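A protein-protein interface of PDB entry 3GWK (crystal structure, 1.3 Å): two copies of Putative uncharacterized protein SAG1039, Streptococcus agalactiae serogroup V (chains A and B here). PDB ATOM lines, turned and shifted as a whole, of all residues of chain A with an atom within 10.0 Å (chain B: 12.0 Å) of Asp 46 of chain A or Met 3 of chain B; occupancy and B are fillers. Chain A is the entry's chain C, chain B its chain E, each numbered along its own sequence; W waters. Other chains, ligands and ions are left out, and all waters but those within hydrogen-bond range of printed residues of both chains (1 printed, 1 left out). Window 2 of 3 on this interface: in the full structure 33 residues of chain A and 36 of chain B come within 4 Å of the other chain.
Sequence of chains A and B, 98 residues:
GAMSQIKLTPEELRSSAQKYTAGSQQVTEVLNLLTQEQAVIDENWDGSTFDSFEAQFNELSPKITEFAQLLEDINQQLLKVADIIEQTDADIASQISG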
ATOM      1  N   ALA A  39     -18.373  23.318  28.046  1.00  0.00           N
ATOM      2  CA  ALA A  39     -18.680  23.029  26.645  1.00  0.00           C
ATOM      3  C   ALA A  39     -18.225  24.167  25.744  1.00  0.00           C
ATOM      4  O   ALA A  39     -17.644  23.931  24.662  1.00  0.00           O
ATOM      5  CB  ALA A  39     -20.205  22.772  26.529  1.00  0.00           C
ATOM      6  N   VAL A  40     -18.414  25.423  26.191  1.00  0.00           N
ATOM      7  CA  VAL A  40     -17.917  26.549  25.431  1.00  0.00           C
ATOM      8  C   VAL A  40     -16.391  26.487  25.257  1.00  0.00           C
ATOM      9  O   VAL A  40     -15.872  26.714  24.157  1.00  0.00           O
ATOM     10  CB  VAL A  40     -18.337  27.913  26.013  1.00  0.00           C
ATOM     11  CG1 VAL A  40     -17.709  29.053  25.223  1.00  0.00           C
ATOM     12  CG2 VAL A  40     -19.863  28.037  26.080  1.00  0.00           C
ATOM     13  N   ILE A  41     -15.690  26.164  26.320  1.00  0.00           N
ATOM     14  CA  ILE A  41     -14.244  26.066  26.243  1.00  0.00           C
ATOM     15  C   ILE A  41     -13.828  24.948  25.317  1.00  0.00           C
ATOM     16  O   ILE A  41     -12.915  25.081  24.488  1.00  0.00           O
ATOM     17  CB  ILE A  41     -13.643  25.899  27.635  1.00  0.00           C
ATOM     18  CG1 ILE A  41     -13.718  27.260  28.391  1.00  0.00           C
ATOM     19  CG2 ILE A  41     -12.146  25.422  27.599  1.00  0.00           C
ATOM     20  CD1 ILE A  41     -13.618  27.192  29.884  1.00  0.00           C
ATOM     21  N   ASP A  42     -14.518  23.850  25.404  1.00  0.00           N
ATOM     22  CA  ASP A  42     -14.182  22.719  24.583  1.00  0.00           C
ATOM     23  C   ASP A  42     -14.317  23.026  23.075  1.00  0.00           C
ATOM     24  O   ASP A  42     -13.500  22.580  22.248  1.00  0.00           O
ATOM     25  CB  ASP A  42     -15.049  21.542  24.995  1.00  0.00           C
ATOM     26  CG  ASP A  42     -14.733  20.282  24.188  1.00  0.00           C
ATOM     27  OD1 ASP A  42     -15.703  19.689  23.656  1.00  0.00           O
ATOM     28  OD2 ASP A  42     -13.521  19.908  24.095  1.00  0.00           O
ATOM     29  N   GLU A  43     -15.354  23.780  22.738  1.00  0.00           N
ATOM     30  CA  GLU A  43     -15.726  24.003  21.359  1.00  0.00           C
ATOM     31  C   GLU A  43     -14.921  25.131  20.770  1.00  0.00           C
ATOM     32  O   GLU A  43     -14.785  25.248  19.541  1.00  0.00           O
ATOM     33  CB  GLU A  43     -17.236  24.348  21.291  1.00  0.00           C
ATOM     34  CG  GLU A  43     -18.071  23.158  21.815  1.00  0.00           C
ATOM     35  CD  GLU A  43     -19.572  23.463  22.058  1.00  0.00           C
ATOM     36  OE1 GLU A  43     -20.023  24.609  21.712  1.00  0.00           O
ATOM     37  OE2 GLU A  43     -20.272  22.533  22.599  1.00  0.00           O
ATOM     38  N   ASN A  44     -14.363  25.983  21.597  1.00  0.00           N
ATOM     39  CA  ASN A  44     -13.914  27.255  21.074  1.00  0.00           C
ATOM     40  C   ASN A  44     -12.506  27.417  21.381  1.00  0.00           C
ATOM     41  O   ASN A  44     -11.912  28.501  21.238  1.00  0.00           O
ATOM     42  CB  ASN A  44     -14.735  28.410  21.624  1.00  0.00           C
ATOM     43  CG  ASN A  44     -16.080  28.482  20.989  1.00  0.00           C
ATOM     44  OD1 ASN A  44     -16.205  28.806  19.803  1.00  0.00           O
ATOM     45  ND2 ASN A  44     -17.107  28.169  21.759  1.00  0.00           N
ATOM     46  N   TRP A  45     -11.915  26.291  21.740  1.00  0.00           N
ATOM     47  CA  TRP A  45     -10.511  26.283  22.010  1.00  0.00           C
ATOM     48  C   TRP A  45     -10.103  24.935  21.527  1.00  0.00           C
ATOM     49  O   TRP A  45     -10.089  23.972  22.311  1.00  0.00           O
ATOM     50  CB  TRP A  45     -10.134  26.438  23.532  1.00  0.00           C
ATOM     51  CG  TRP A  45      -8.650  26.426  23.796  1.00  0.00           C
ATOM     52  CD1 TRP A  45      -7.650  26.464  22.891  1.00  0.00           C
ATOM     53  CD2 TRP A  45      -8.072  26.580  25.055  1.00  0.00           C
ATOM     54  NE1 TRP A  45      -6.453  26.532  23.546  1.00  0.00           N
ATOM     55  CE2 TRP A  45      -6.703  26.610  24.881  1.00  0.00           C
ATOM     56  CE3 TRP A  45      -8.580  26.654  26.358  1.00  0.00           C
ATOM     57  CZ2 TRP A  45      -5.834  26.694  25.937  1.00  0.00           C
ATOM     58  CZ3 TRP A  45      -7.739  26.817  27.361  1.00  0.00           C
ATOM     59  CH2 TRP A  45      -6.393  26.788  27.168  1.00  0.00           C
ATOM     60  N   ASP A  46      -9.619  24.893  20.300  1.00  0.00           N
ATOM     61  CA  ASP A  46      -9.242  23.600  19.723  1.00  0.00           C
ATOM     62  C   ASP A  46      -7.943  23.102  20.291  1.00  0.00           C
ATOM     63  O   ASP A  46      -7.053  23.915  20.673  1.00  0.00           O
ATOM     64  CB  ASP A  46      -9.133  23.642  18.186  1.00  0.00           C
ATOM     65  CG  ASP A  46      -8.711  22.290  17.579  1.00  0.00           C
ATOM     66  OD1 ASP A  46      -7.518  21.921  17.677  1.00  0.00           O
ATOM     67  OD2 ASP A  46      -9.577  21.603  16.984  1.00  0.00           O
ATOM     68  N   GLY A  47      -7.803  21.782  20.360  1.00  0.00           N
ATOM     69  CA  GLY A  47      -6.602  21.128  20.864  1.00  0.00           C
ATOM     70  C   GLY A  47      -6.786  20.399  22.224  1.00  0.00           C
ATOM     71  O   GLY A  47      -7.972  20.269  22.704  1.00  0.00           O
ATOM     72  N   SER A  48      -5.661  20.002  22.895  1.00  0.00           N
ATOM     73  CA  SER A  48      -5.695  19.223  24.201  1.00  0.00           C
ATOM     74  C   SER A  48      -5.291  19.943  25.476  1.00  0.00           C
ATOM     75  O   SER A  48      -5.138  19.321  26.549  1.00  0.00           O
ATOM     76  CB  SER A  48      -4.749  18.034  24.157  1.00  0.00           C
ATOM     77  OG  SER A  48      -3.393  18.454  23.947  1.00  0.00           O
ATOM     78  N   THR A  49      -5.155  21.239  25.379  1.00  0.00           N
ATOM     79  CA  THR A  49      -4.683  21.984  26.532  1.00  0.00           C
ATOM     80  C   THR A  49      -5.468  21.729  27.842  1.00  0.00           C
ATOM     81  O   THR A  49      -4.866  21.591  28.882  1.00  0.00           O
ATOM     82  CB  THR A  49      -4.604  23.484  26.214  1.00  0.00           C
ATOM     83  OG1 THR A  49      -3.901  23.679  24.990  1.00  0.00           O
ATOM     84  CG2 THR A  49      -3.870  24.234  27.353  1.00  0.00           C
ATOM     85  N   PHE A  50      -6.791  21.690  27.777  1.00  0.00           N
ATOM     86  CA  PHE A  50      -7.588  21.497  28.999  1.00  0.00           C
ATOM     87  C   PHE A  50      -8.142  20.079  29.112  1.00  0.00           C
ATOM     88  O   PHE A  50      -9.117  19.846  29.796  1.00  0.00           O
ATOM     89  CB  PHE A  50      -8.698  22.511  29.055  1.00  0.00           C
ATOM     90  CG  PHE A  50      -8.320  23.802  29.766  1.00  0.00           C
ATOM     91  CD1 PHE A  50      -7.020  24.201  29.952  1.00  0.00           C
ATOM     92  CD2 PHE A  50      -9.311  24.627  30.234  1.00  0.00           C
ATOM     93  CE1 PHE A  50      -6.731  25.443  30.602  1.00  0.00           C
ATOM     94  CE2 PHE A  50      -9.008  25.811  30.886  1.00  0.00           C
ATOM     95  CZ  PHE A  50      -7.743  26.205  31.072  1.00  0.00           C
ATOM     96  N   ASP A  51      -7.502  19.097  28.474  1.00  0.00           N
ATOM     97  CA  ASP A  51      -8.035  17.739  28.501  1.00  0.00           C
ATOM     98  C   ASP A  51      -8.059  17.133  29.886  1.00  0.00           C
ATOM     99  O   ASP A  51      -8.996  16.375  30.225  1.00  0.00           O
ATOM    100  CB  ASP A  51      -7.254  16.764  27.567  1.00  0.00           C
ATOM    101  CG  ASP A  51      -7.561  16.962  26.098  1.00  0.00           C
ATOM    102  OD1 ASP A  51      -8.304  17.883  25.733  1.00  0.00           O
ATOM    103  OD2 ASP A  51      -7.027  16.157  25.298  1.00  0.00           O
ATOM    104  N   ALA B   2      -3.630  19.988  14.009  1.00  0.00           N
ATOM    105  CA  ALA B   2      -3.843  20.911  15.130  1.00  0.00           C
ATOM    106  C   ALA B   2      -3.907  22.375  14.660  1.00  0.00           C
ATOM    107  O   ALA B   2      -2.936  22.911  14.096  1.00  0.00           O
ATOM    108  CB  ALA B   2      -2.712  20.776  16.193  1.00  0.00           C
ATOM    109  N   MET B   3      -5.036  23.037  14.899  1.00  0.00           N
ATOM    110  CA  MET B   3      -5.094  24.435  14.609  1.00  0.00           C
ATOM    111  C   MET B   3      -4.440  25.114  15.791  1.00  0.00           C
ATOM    112  O   MET B   3      -4.613  24.699  16.979  1.00  0.00           O
ATOM    113  CB  MET B   3      -6.512  24.960  14.476  1.00  0.00           C
ATOM    114  CG  MET B   3      -7.342  24.696  15.606  1.00  0.00           C
ATOM    115  SD  MET B   3      -9.026  25.491  15.309  1.00  0.00           S
ATOM    116  CE  MET B   3      -9.976  24.148  14.454  1.00  0.00           C
ATOM    117  N   SER B   4      -3.848  26.234  15.458  1.00  0.00           N
ATOM    118  CA  SER B   4      -3.335  27.167  16.506  1.00  0.00           C
ATOM    119  C   SER B   4      -4.406  28.112  17.024  1.00  0.00           C
ATOM    120  O   SER B   4      -4.281  28.654  18.097  1.00  0.00           O
ATOM    121  CB  SER B   4      -2.157  27.965  15.887  1.00  0.00           C
ATOM    122  OG  SER B   4      -1.096  27.141  15.511  1.00  0.00           O
ATOM    123  N   GLN B   5      -5.369  28.404  16.190  1.00  0.00           N
ATOM    124  CA  GLN B   5      -6.415  29.347  16.507  1.00  0.00           C
ATOM    125  C   GLN B   5      -7.099  28.994  17.811  1.00  0.00           C
ATOM    126  O   GLN B   5      -7.369  27.801  18.094  1.00  0.00           O
ATOM    127  CB  GLN B   5      -7.473  29.337  15.400  1.00  0.00           C
ATOM    128  CG  GLN B   5      -8.574  30.352  15.530  1.00  0.00           C
ATOM    129  CD  GLN B   5      -9.601  30.167  14.478  1.00  0.00           C
ATOM    130  OE1 GLN B   5      -9.853  29.055  14.021  1.00  0.00           O
ATOM    131  NE2 GLN B   5     -10.295  31.251  14.178  1.00  0.00           N
ATOM    132  N   ILE B   6      -7.356  30.075  18.571  1.00  0.00           N
ATOM    133  CA  ILE B   6      -8.119  29.992  19.851  1.00  0.00           C
ATOM    134  C   ILE B   6      -9.247  30.981  19.693  1.00  0.00           C
ATOM    135  O   ILE B   6      -9.012  32.188  19.653  1.00  0.00           O
ATOM    136  CB  ILE B   6      -7.246  30.321  21.065  1.00  0.00           C
ATOM    137  CG1 ILE B   6      -6.061  29.368  21.103  1.00  0.00           C
ATOM    138  CG2 ILE B   6      -8.117  30.352  22.353  1.00  0.00           C
ATOM    139  CD1 ILE B   6      -5.012  29.660  22.191  1.00  0.00           C
ATOM    140  N   LYS B   7     -10.485  30.497  19.612  1.00  0.00           N
ATOM    141  CA  LYS B   7     -11.589  31.366  19.253  1.00  0.00           C
ATOM    142  C   LYS B   7     -12.010  32.317  20.367  1.00  0.00           C
ATOM    143  O   LYS B   7     -12.401  33.457  20.095  1.00  0.00           O
ATOM    144  CB  LYS B   7     -12.805  30.579  18.732  1.00  0.00           C
ATOM    145  CG  LYS B   7     -12.465  29.896  17.480  1.00  0.00           C
ATOM    146  CD  LYS B   7     -13.630  28.984  17.019  1.00  0.00           C
ATOM    147  CE  LYS B   7     -13.184  28.089  15.879  1.00  0.00           C
ATOM    148  NZ  LYS B   7     -14.356  27.439  15.270  1.00  0.00           N
ATOM    149  N   LEU B   8     -11.881  31.894  21.628  1.00  0.00           N
ATOM    150  CA  LEU B   8     -12.217  32.768  22.741  1.00  0.00           C
ATOM    151  C   LEU B   8     -11.125  33.806  22.922  1.00  0.00           C
ATOM    152  O   LEU B   8      -9.931  33.461  23.020  1.00  0.00           O
ATOM    153  CB  LEU B   8     -12.342  31.989  24.067  1.00  0.00           C
ATOM    154  CG  LEU B   8     -13.430  30.885  24.074  1.00  0.00           C
ATOM    155  CD1 LEU B   8     -13.459  30.022  25.294  1.00  0.00           C
ATOM    156  CD2 LEU B   8     -14.757  31.561  24.083  1.00  0.00           C
ATOM    157  N   THR B   9     -11.548  35.059  22.930  1.00  0.00           N
ATOM    158  CA  THR B   9     -10.669  36.185  23.171  1.00  0.00           C
ATOM    159  C   THR B   9     -10.203  36.246  24.672  1.00  0.00           C
ATOM    160  O   THR B   9     -10.818  35.654  25.536  1.00  0.00           O
ATOM    161  CB  THR B   9     -11.302  37.488  22.831  1.00  0.00           C
ATOM    162  OG1 THR B   9     -12.352  37.757  23.796  1.00  0.00           O
ATOM    163  CG2 THR B   9     -11.932  37.494  21.371  1.00  0.00           C
ATOM    164  N   GLU B  12     -13.070  37.175  26.765  1.00  0.00           N
ATOM    165  CA  GLU B  12     -14.013  36.082  26.917  1.00  0.00           C
ATOM    166  C   GLU B  12     -13.508  35.023  27.867  1.00  0.00           C
ATOM    167  O   GLU B  12     -14.247  34.464  28.718  1.00  0.00           O
ATOM    168  CB  GLU B  12     -14.407  35.468  25.581  1.00  0.00           C
ATOM    169  CG  GLU B  12     -15.237  36.404  24.681  1.00  0.00           C
ATOM    170  CD  GLU B  12     -15.406  35.902  23.276  1.00  0.00           C
ATOM    171  OE1 GLU B  12     -14.482  35.284  22.771  1.00  0.00           O
ATOM    172  OE2 GLU B  12     -16.506  36.169  22.694  1.00  0.00           O
ATOM    173  N   LEU B  13     -12.212  34.722  27.754  1.00  0.00           N
ATOM    174  CA  LEU B  13     -11.610  33.783  28.707  1.00  0.00           C
ATOM    175  C   LEU B  13     -11.671  34.281  30.160  1.00  0.00           C
ATOM    176  O   LEU B  13     -11.947  33.524  31.098  1.00  0.00           O
ATOM    177  CB  LEU B  13     -10.129  33.504  28.329  1.00  0.00           C
ATOM    178  CG  LEU B  13      -9.880  32.734  27.006  1.00  0.00           C
ATOM    179  CD1 LEU B  13      -8.506  32.907  26.485  1.00  0.00           C
ATOM    180  CD2 LEU B  13     -10.216  31.336  27.185  1.00  0.00           C
ATOM    181  N   LEU B  78      -7.090  29.669  33.068  1.00  0.00           N
ATOM    182  CA  LEU B  78      -7.761  30.549  32.083  1.00  0.00           C
ATOM    183  C   LEU B  78      -7.160  31.968  32.118  1.00  0.00           C
ATOM    184  O   LEU B  78      -6.944  32.560  31.067  1.00  0.00           O
ATOM    185  CB  LEU B  78      -9.259  30.615  32.323  1.00  0.00           C
ATOM    186  CG  LEU B  78     -10.074  29.388  31.902  1.00  0.00           C
ATOM    187  CD1 LEU B  78     -11.513  29.552  32.513  1.00  0.00           C
ATOM    188  CD2 LEU B  78     -10.129  29.294  30.383  1.00  0.00           C
ATOM    189  N   VAL B  81      -3.725  31.770  30.413  1.00  0.00           N
ATOM    190  CA  VAL B  81      -3.775  31.668  28.980  1.00  0.00           C
ATOM    191  C   VAL B  81      -4.225  32.980  28.355  1.00  0.00           C
ATOM    192  O   VAL B  81      -3.718  33.389  27.299  1.00  0.00           O
ATOM    193  CB  VAL B  81      -4.702  30.559  28.513  1.00  0.00           C
ATOM    194  CG1 VAL B  81      -4.452  30.399  26.950  1.00  0.00           C
ATOM    195  CG2 VAL B  81      -4.374  29.318  29.205  1.00  0.00           C
ATOM    196  N   ILE B  85      -2.265  35.008  25.399  1.00  0.00           N
ATOM    197  CA  ILE B  85      -2.915  35.409  24.157  1.00  0.00           C
ATOM    198  C   ILE B  85      -2.934  36.901  23.976  1.00  0.00           C
ATOM    199  O   ILE B  85      -2.720  37.394  22.890  1.00  0.00           O
ATOM    200  CB  ILE B  85      -4.306  34.800  24.088  1.00  0.00           C
ATOM    201  CG1 ILE B  85      -4.243  33.278  24.044  1.00  0.00           C
ATOM    202  CG2 ILE B  85      -5.077  35.386  22.927  1.00  0.00           C
ATOM    203  CD1 ILE B  85      -5.617  32.576  24.318  1.00  0.00           C
HETATM  204  O   HOH W   1     -10.083  27.448  18.646  1.00  0.00           O
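No position is printed for both chains.
Of the 7 pairs that touch across the chains among the printed residues, none has its exchanged pair printed and touching as well.
Water W1 lies within hydrogen-bond range of the backbone carbonyl oxygen (O) of Gln 5 of chain B, the backbone NH (N) of Asp 46 of chain A, the backbone NH (N) of Lys 7 of chain B and the backbone carbonyl oxygen (O) of Asn 44 of chain A.
Among the printed residues, merely in contact across the chains: Asp 46 of chain A with Met 3 of chain B, Phe 50 of chain A with Leu 78 of chain B, Trp 45 of chain A with Ile 6 of chain B, Trp 45 of chain A with Val 81 of chain B and Asn 44 of chain A with Ile 6 of chain B.
N of Leu 8 of chain B lies within hydrogen-bond range of O of Asn 44 of chain A, at 3.4 Å.
N of Lys 7 of chain B lies within hydrogen-bond range of O of Asn 44 of chain A, 2.9 Å away.
Printed residues of chain B within 4 Å of Asp 46 of chain A: Met 3 (3.3 Å).
Of the printed residues of chain A, Met 3 of chain B touches Asp 46 (3.3 Å).
No residue of chain B comes within 4 Å of Gly 47 of chain A.
No residue of chain A comes within 4 Å of Ser 4 of chain B.
Printed residues of chain B within 4 Å of Asn 44 of chain A: Ile 6, Lys 7 and Leu 8.
Of the printed residues of chain A, Leu 8 of chain B touches Asn 44.
Of the printed residues of chain A, Ile 6 of chain B touches Asn 44 and Trp 45.
Of the printed residues of chain A, Val 81 of chain B touches Trp 45 (3.8 Å).
Val 40 of chain A touches none of the printed residues of chain B.
The nearest printed residue of chain B that does not touch Asp 46 of chain A is Gln 5 of chain B (4.3 Å).
The nearest printed residue of chain A that does not touch Met 3 of chain B is Gly 47 of chain A (5.5 Å).
The backbone carbonyl oxygen of Val 40 of chain A is in hydrogen-bond range of the side-chain amide nitrogen of Asn 44 of chain A (3.1 Å).
Of the 13 printed residues of chain A, 4 touch a printed residue of chain B.
Hydrophobic or aromatic side chains of chain A within 4 Å of the printed part of chain B: Trp 45 and Phe 50.
Hydrophobic or aromatic side chains of chain B that line the printed part of chain A: Met 3, Ile 6, Leu 8, Leu 78 and Val 81.
Among the printed residues, 7 pairs touch across the chains.
Among the printed residues, no Asp or Glu carboxylate lies within 4 Å of a Lys or Arg side-chain nitrogen of the other chain.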
